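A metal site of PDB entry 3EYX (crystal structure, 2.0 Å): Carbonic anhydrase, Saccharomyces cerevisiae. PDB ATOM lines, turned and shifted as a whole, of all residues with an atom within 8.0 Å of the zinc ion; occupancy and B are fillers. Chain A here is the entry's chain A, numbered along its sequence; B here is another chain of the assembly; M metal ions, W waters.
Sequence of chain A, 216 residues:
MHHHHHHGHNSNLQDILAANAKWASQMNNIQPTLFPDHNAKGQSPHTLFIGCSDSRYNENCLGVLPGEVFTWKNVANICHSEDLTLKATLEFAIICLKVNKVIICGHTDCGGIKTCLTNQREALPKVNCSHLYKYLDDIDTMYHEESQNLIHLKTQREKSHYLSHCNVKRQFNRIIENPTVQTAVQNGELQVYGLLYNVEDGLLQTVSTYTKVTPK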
ATOM      1  N   GLY A  51      -5.575  12.057  27.882  1.00  0.00           N
ATOM      2  CA  GLY A  51      -5.655  12.602  26.537  1.00  0.00           C
ATOM      3  C   GLY A  51      -6.428  13.897  26.490  1.00  0.00           C
ATOM      4  O   GLY A  51      -7.002  14.335  27.485  1.00  0.00           O
ATOM      5  N   CYS A  52      -6.420  14.515  25.313  1.00  0.00           N
ATOM      6  CA  CYS A  52      -7.112  15.766  25.136  1.00  0.00           C
ATOM      7  C   CYS A  52      -8.613  15.511  25.040  1.00  0.00           C
ATOM      8  O   CYS A  52      -9.027  14.451  24.572  1.00  0.00           O
ATOM      9  CB  CYS A  52      -6.624  16.468  23.876  1.00  0.00           C
ATOM     10  SG  CYS A  52      -7.330  18.087  23.695  1.00  0.00           S
ATOM     11  N   SER A  53      -9.406  16.494  25.458  1.00  0.00           N
ATOM     12  CA  SER A  53     -10.868  16.447  25.329  1.00  0.00           C
ATOM     13  C   SER A  53     -11.338  16.391  23.872  1.00  0.00           C
ATOM     14  O   SER A  53     -12.496  16.044  23.606  1.00  0.00           O
ATOM     15  CB  SER A  53     -11.505  17.646  26.030  1.00  0.00           C
ATOM     16  OG  SER A  53     -11.242  17.637  27.421  1.00  0.00           O
ATOM     17  N   ASP A  54     -10.454  16.748  22.944  1.00  0.00           N
ATOM     18  CA  ASP A  54     -10.731  16.674  21.506  1.00  0.00           C
ATOM     19  C   ASP A  54     -11.644  15.509  21.116  1.00  0.00           C
ATOM     20  O   ASP A  54     -11.401  14.358  21.468  1.00  0.00           O
ATOM     21  CB  ASP A  54      -9.406  16.603  20.719  1.00  0.00           C
ATOM     22  CG  ASP A  54      -9.598  16.934  19.234  1.00  0.00           C
ATOM     23  OD1 ASP A  54     -10.196  16.129  18.502  1.00  0.00           O
ATOM     24  OD2 ASP A  54      -9.126  18.001  18.821  1.00  0.00           O
ATOM     25  N   SER A  55     -12.685  15.836  20.344  1.00  0.00           N
ATOM     26  CA  SER A  55     -13.743  14.883  19.965  1.00  0.00           C
ATOM     27  C   SER A  55     -13.311  13.791  19.007  1.00  0.00           C
ATOM     28  O   SER A  55     -14.052  12.826  18.793  1.00  0.00           O
ATOM     29  CB  SER A  55     -14.936  15.637  19.360  1.00  0.00           C
ATOM     30  OG  SER A  55     -14.584  16.199  18.102  1.00  0.00           O
ATOM     31  N   ARG A  56     -12.127  13.929  18.428  1.00  0.00           N
ATOM     32  CA  ARG A  56     -11.697  13.069  17.337  1.00  0.00           C
ATOM     33  C   ARG A  56     -11.051  11.779  17.805  1.00  0.00           C
ATOM     34  O   ARG A  56     -10.920  10.836  17.026  1.00  0.00           O
ATOM     35  CB  ARG A  56     -10.795  13.825  16.359  1.00  0.00           C
ATOM     36  CG  ARG A  56     -11.599  14.801  15.492  1.00  0.00           C
ATOM     37  CD  ARG A  56     -10.698  15.776  14.743  1.00  0.00           C
ATOM     38  NE  ARG A  56      -9.918  16.613  15.652  1.00  0.00           N
ATOM     39  CZ  ARG A  56      -8.995  17.500  15.256  1.00  0.00           C
ATOM     40  NH1 ARG A  56      -8.747  17.667  13.962  1.00  0.00           N
ATOM     41  NH2 ARG A  56      -8.327  18.217  16.159  1.00  0.00           N
ATOM     42  N   TYR A  57     -10.662  11.729  19.079  1.00  0.00           N
ATOM     43  CA  TYR A  57     -10.093  10.520  19.631  1.00  0.00           C
ATOM     44  C   TYR A  57     -10.371  10.363  21.121  1.00  0.00           C
ATOM     45  O   TYR A  57     -10.795  11.301  21.795  1.00  0.00           O
ATOM     46  CB  TYR A  57      -8.570  10.445  19.346  1.00  0.00           C
ATOM     47  CG  TYR A  57      -7.681  11.245  20.271  1.00  0.00           C
ATOM     48  CD1 TYR A  57      -6.632  10.637  20.951  1.00  0.00           C
ATOM     49  CD2 TYR A  57      -7.878  12.631  20.463  1.00  0.00           C
ATOM     50  CE1 TYR A  57      -5.795  11.357  21.796  1.00  0.00           C
ATOM     51  CE2 TYR A  57      -7.053  13.360  21.316  1.00  0.00           C
ATOM     52  CZ  TYR A  57      -6.014  12.717  21.975  1.00  0.00           C
ATOM     53  OH  TYR A  57      -5.178  13.432  22.811  1.00  0.00           O
ATOM     54  N   ASN A  74      -8.862  15.926  29.239  1.00  0.00           N
ATOM     55  CA  ASN A  74      -8.970  17.355  29.518  1.00  0.00           C
ATOM     56  C   ASN A  74      -8.414  18.225  28.392  1.00  0.00           C
ATOM     57  O   ASN A  74      -7.622  17.747  27.570  1.00  0.00           O
ATOM     58  CB  ASN A  74      -8.357  17.735  30.874  1.00  0.00           C
ATOM     59  CG  ASN A  74      -6.823  17.724  30.889  1.00  0.00           C
ATOM     60  OD1 ASN A  74      -6.176  18.447  30.132  1.00  0.00           O
ATOM     61  ND2 ASN A  74      -6.234  16.933  31.780  1.00  0.00           N
ATOM     62  N   VAL A  75      -8.815  19.492  28.365  1.00  0.00           N
ATOM     63  CA  VAL A  75      -8.380  20.409  27.311  1.00  0.00           C
ATOM     64  C   VAL A  75      -6.854  20.438  27.229  1.00  0.00           C
ATOM     65  O   VAL A  75      -6.174  20.751  28.205  1.00  0.00           O
ATOM     66  CB  VAL A  75      -8.995  21.820  27.471  1.00  0.00           C
ATOM     67  CG1 VAL A  75      -8.365  22.827  26.465  1.00  0.00           C
ATOM     68  CG2 VAL A  75     -10.513  21.768  27.294  1.00  0.00           C
ATOM     69  N   ALA A  76      -6.336  20.055  26.059  1.00  0.00           N
ATOM     70  CA  ALA A  76      -4.883  20.029  25.767  1.00  0.00           C
ATOM     71  C   ALA A  76      -4.047  19.096  26.657  1.00  0.00           C
ATOM     72  O   ALA A  76      -2.830  19.312  26.830  1.00  0.00           O
ATOM     73  CB  ALA A  76      -4.303  21.465  25.723  1.00  0.00           C
ATOM     74  N   ASN A  77      -4.669  18.057  27.204  1.00  0.00           N
ATOM     75  CA  ASN A  77      -3.986  17.082  28.088  1.00  0.00           C
ATOM     76  C   ASN A  77      -2.905  17.680  29.021  1.00  0.00           C
ATOM     77  O   ASN A  77      -1.774  17.189  29.078  1.00  0.00           O
ATOM     78  CB  ASN A  77      -3.473  15.856  27.282  1.00  0.00           C
ATOM     79  CG  ASN A  77      -2.702  16.237  26.012  1.00  0.00           C
ATOM     80  OD1 ASN A  77      -3.296  16.437  24.943  1.00  0.00           O
ATOM     81  ND2 ASN A  77      -1.375  16.308  26.117  1.00  0.00           N
ATOM     82  N   CYS A 105      -1.259  10.832  26.143  1.00  0.00           N
ATOM     83  CA  CYS A 105      -1.450  10.824  24.708  1.00  0.00           C
ATOM     84  C   CYS A 105      -2.003  12.139  24.184  1.00  0.00           C
ATOM     85  O   CYS A 105      -3.194  12.426  24.307  1.00  0.00           O
ATOM     86  CB  CYS A 105      -2.364   9.664  24.301  1.00  0.00           C
ATOM     87  SG  CYS A 105      -2.516   9.346  22.543  1.00  0.00           S
ATOM     88  N   GLY A 106      -1.114  12.936  23.608  1.00  0.00           N
ATOM     89  CA  GLY A 106      -1.527  14.152  22.920  1.00  0.00           C
ATOM     90  C   GLY A 106      -1.970  13.812  21.514  1.00  0.00           C
ATOM     91  O   GLY A 106      -2.097  12.647  21.174  1.00  0.00           O
ATOM     92  N   HIS A 107      -2.223  14.839  20.701  1.00  0.00           N
ATOM     93  CA  HIS A 107      -2.627  14.642  19.328  1.00  0.00           C
ATOM     94  C   HIS A 107      -2.255  15.845  18.465  1.00  0.00           C
ATOM     95  O   HIS A 107      -2.046  16.954  18.960  1.00  0.00           O
ATOM     96  CB  HIS A 107      -4.140  14.395  19.241  1.00  0.00           C
ATOM     97  CG  HIS A 107      -4.955  15.615  19.540  1.00  0.00           C
ATOM     98  ND1 HIS A 107      -5.593  16.344  18.567  1.00  0.00           N
ATOM     99  CD2 HIS A 107      -5.198  16.251  20.711  1.00  0.00           C
ATOM    100  CE1 HIS A 107      -6.213  17.369  19.116  1.00  0.00           C
ATOM    101  NE2 HIS A 107      -5.985  17.335  20.418  1.00  0.00           N
ATOM    102  N   THR A 108      -2.172  15.600  17.151  1.00  0.00           N
ATOM    103  CA  THR A 108      -1.909  16.638  16.173  1.00  0.00           C
ATOM    104  C   THR A 108      -3.164  17.478  15.973  1.00  0.00           C
ATOM    105  O   THR A 108      -4.281  16.982  16.155  1.00  0.00           O
ATOM    106  CB  THR A 108      -1.495  16.037  14.813  1.00  0.00           C
ATOM    107  OG1 THR A 108      -2.536  15.163  14.365  1.00  0.00           O
ATOM    108  CG2 THR A 108      -0.181  15.244  14.922  1.00  0.00           C
ATOM    109  N   ASP A 109      -2.963  18.735  15.580  1.00  0.00           N
ATOM    110  CA  ASP A 109      -4.060  19.652  15.264  1.00  0.00           C
ATOM    111  C   ASP A 109      -4.860  19.956  16.542  1.00  0.00           C
ATOM    112  O   ASP A 109      -6.094  19.940  16.539  1.00  0.00           O
ATOM    113  CB  ASP A 109      -4.947  19.071  14.125  1.00  0.00           C
ATOM    114  CG  ASP A 109      -5.993  20.046  13.619  1.00  0.00           C
ATOM    115  OD1 ASP A 109      -5.685  21.245  13.495  1.00  0.00           O
ATOM    116  OD2 ASP A 109      -7.134  19.607  13.345  1.00  0.00           O
ATOM    117  N   CYS A 110      -4.149  20.220  17.640  1.00  0.00           N
ATOM    118  CA  CYS A 110      -4.757  20.454  18.952  1.00  0.00           C
ATOM    119  C   CYS A 110      -5.199  21.907  19.087  1.00  0.00           C
ATOM    120  O   CYS A 110      -4.378  22.817  18.947  1.00  0.00           O
ATOM    121  CB  CYS A 110      -3.809  20.074  20.089  1.00  0.00           C
ATOM    122  SG  CYS A 110      -4.528  20.189  21.785  1.00  0.00           S
ATOM    123  N   GLY A 111      -6.486  22.118  19.360  1.00  0.00           N
ATOM    124  CA  GLY A 111      -7.080  23.449  19.448  1.00  0.00           C
ATOM    125  C   GLY A 111      -6.341  24.411  20.357  1.00  0.00           C
ATOM    126  O   GLY A 111      -6.025  25.526  19.945  1.00  0.00           O
ATOM    127  N   GLY A 112      -6.056  23.971  21.580  1.00  0.00           N
ATOM    128  CA  GLY A 112      -5.353  24.788  22.576  1.00  0.00           C
ATOM    129  C   GLY A 112      -3.973  25.230  22.135  1.00  0.00           C
ATOM    130  O   GLY A 112      -3.584  26.392  22.333  1.00  0.00           O
ATOM    131  N   ILE A 113      -3.227  24.307  21.537  1.00  0.00           N
ATOM    132  CA  ILE A 113      -1.903  24.617  21.007  1.00  0.00           C
ATOM    133  C   ILE A 113      -1.966  25.632  19.842  1.00  0.00           C
ATOM    134  O   ILE A 113      -1.247  26.625  19.831  1.00  0.00           O
ATOM    135  CB  ILE A 113      -1.131  23.324  20.647  1.00  0.00           C
ATOM    136  CG1 ILE A 113      -0.877  22.487  21.922  1.00  0.00           C
ATOM    137  CG2 ILE A 113       0.188  23.651  19.948  1.00  0.00           C
ATOM    138  CD1 ILE A 113      -0.448  21.052  21.684  1.00  0.00           C
ATOM    139  N   LYS A 114      -2.871  25.387  18.882  1.00  0.00           N
ATOM    140  CA  LYS A 114      -3.090  26.294  17.752  1.00  0.00           C
ATOM    141  C   LYS A 114      -3.414  27.730  18.184  1.00  0.00           C
ATOM    142  O   LYS A 114      -2.883  28.691  17.619  1.00  0.00           O
ATOM    143  CB  LYS A 114      -4.206  25.759  16.856  1.00  0.00           C
ATOM    144  CG  LYS A 114      -3.743  24.744  15.829  1.00  0.00           C
ATOM    145  CD  LYS A 114      -4.865  23.832  15.367  1.00  0.00           C
ATOM    146  CE  LYS A 114      -5.911  24.588  14.554  1.00  0.00           C
ATOM    147  NZ  LYS A 114      -7.027  23.669  14.174  1.00  0.00           N
ATOM    148  N   SER A 164       2.623  20.030  19.339  1.00  0.00           N
ATOM    149  CA  SER A 164       1.834  18.906  19.825  1.00  0.00           C
ATOM    150  C   SER A 164       2.747  17.809  20.409  1.00  0.00           C
ATOM    151  O   SER A 164       2.491  17.272  21.480  1.00  0.00           O
ATOM    152  CB  SER A 164       0.959  18.336  18.713  1.00  0.00           C
ATOM    153  OG  SER A 164      -0.262  19.052  18.603  1.00  0.00           O
ATOM    154  N   ASN A 167       4.340  19.173  23.513  1.00  0.00           N
ATOM    155  CA  ASN A 167       3.440  19.179  24.663  1.00  0.00           C
ATOM    156  C   ASN A 167       3.367  17.784  25.330  1.00  0.00           C
ATOM    157  O   ASN A 167       3.211  17.677  26.553  1.00  0.00           O
ATOM    158  CB  ASN A 167       2.046  19.665  24.272  1.00  0.00           C
ATOM    159  CG  ASN A 167       1.140  19.911  25.466  1.00  0.00           C
ATOM    160  OD1 ASN A 167       1.579  20.394  26.509  1.00  0.00           O
ATOM    161  ND2 ASN A 167      -0.133  19.585  25.317  1.00  0.00           N
ATOM    162  N   VAL A 199      -4.336  12.692  13.941  1.00  0.00           N
ATOM    163  CA  VAL A 199      -5.764  12.734  13.601  1.00  0.00           C
ATOM    164  C   VAL A 199      -6.052  12.319  12.151  1.00  0.00           C
ATOM    165  O   VAL A 199      -7.140  11.842  11.828  1.00  0.00           O
ATOM    166  CB  VAL A 199      -6.389  14.140  13.897  1.00  0.00           C
ATOM    167  CG1 VAL A 199      -6.326  14.460  15.389  1.00  0.00           C
ATOM    168  CG2 VAL A 199      -5.733  15.268  13.062  1.00  0.00           C
ATOM    169  N   PHE B  70     -17.159  16.324  22.362  1.00  0.00           N
ATOM    170  CA  PHE B  70     -16.007  16.827  23.092  1.00  0.00           C
ATOM    171  C   PHE B  70     -16.184  16.420  24.574  1.00  0.00           C
ATOM    172  O   PHE B  70     -17.251  16.618  25.141  1.00  0.00           O
ATOM    173  CB  PHE B  70     -16.000  18.342  22.946  1.00  0.00           C
ATOM    174  CG  PHE B  70     -14.745  19.015  23.397  1.00  0.00           C
ATOM    175  CD1 PHE B  70     -13.599  18.984  22.609  1.00  0.00           C
ATOM    176  CD2 PHE B  70     -14.717  19.725  24.597  1.00  0.00           C
ATOM    177  CE1 PHE B  70     -12.449  19.627  23.019  1.00  0.00           C
ATOM    178  CE2 PHE B  70     -13.566  20.368  25.006  1.00  0.00           C
ATOM    179  CZ  PHE B  70     -12.424  20.321  24.220  1.00  0.00           C
ATOM    180  N   PHE B  92     -14.689  27.097  26.345  1.00  0.00           N
ATOM    181  CA  PHE B  92     -14.236  26.588  25.058  1.00  0.00           C
ATOM    182  C   PHE B  92     -15.352  25.886  24.283  1.00  0.00           C
ATOM    183  O   PHE B  92     -15.552  26.148  23.103  1.00  0.00           O
ATOM    184  CB  PHE B  92     -13.037  25.637  25.205  1.00  0.00           C
ATOM    185  CG  PHE B  92     -12.518  25.142  23.890  1.00  0.00           C
ATOM    186  CD1 PHE B  92     -12.027  26.039  22.942  1.00  0.00           C
ATOM    187  CD2 PHE B  92     -12.528  23.781  23.586  1.00  0.00           C
ATOM    188  CE1 PHE B  92     -11.543  25.587  21.706  1.00  0.00           C
ATOM    189  CE2 PHE B  92     -12.045  23.318  22.359  1.00  0.00           C
ATOM    190  CZ  PHE B  92     -11.545  24.225  21.414  1.00  0.00           C
HETATM  191 ZN    ZN M   1      -6.328  18.857  21.727  1.00  0.00          ZN
HETATM  192  O   HOH W   1      -7.946  19.710  20.536  1.00  0.00           O
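Water W1 bridges the side-chain carboxylate (OD2) of Asp 54 (2.7 Å) and the backbone NH (N) of Gly 111 (3.1 Å).
N of Ala 76 lies close to SG of Cys 52, 3.2 Å away. The backbone NH (N) of Cys 52 lies within hydrogen-bond range of the side-chain hydroxyl (OH) of Tyr 57 (3.0 Å). The side-chain sulfur of Cys 52 sits close to the backbone NH of Asp 54 (3.5 Å). OD2 of Asp 54 is in salt-bridge range of NH2 of Arg 56. The backbone carbonyl oxygen (O) of His 107 sits at hydrogen-bond distance from the side-chain hydroxyl (OG) of Ser 164 (2.8 Å).
NE2 of His 107 binds the zinc ion (2.0 Å). The zinc ion is bound by water W1, at 2.2 Å. The zinc ion is bound by the side-chain sulfur (SG) of Cys 110 (2.2 Å). The zinc ion is bound by SG of Cys 52 (2.3 Å).
Asp 54 touches the zinc ion. Within 4 Å of the zinc ion: Cys 52, Asp 54, His 107 and Cys 110.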
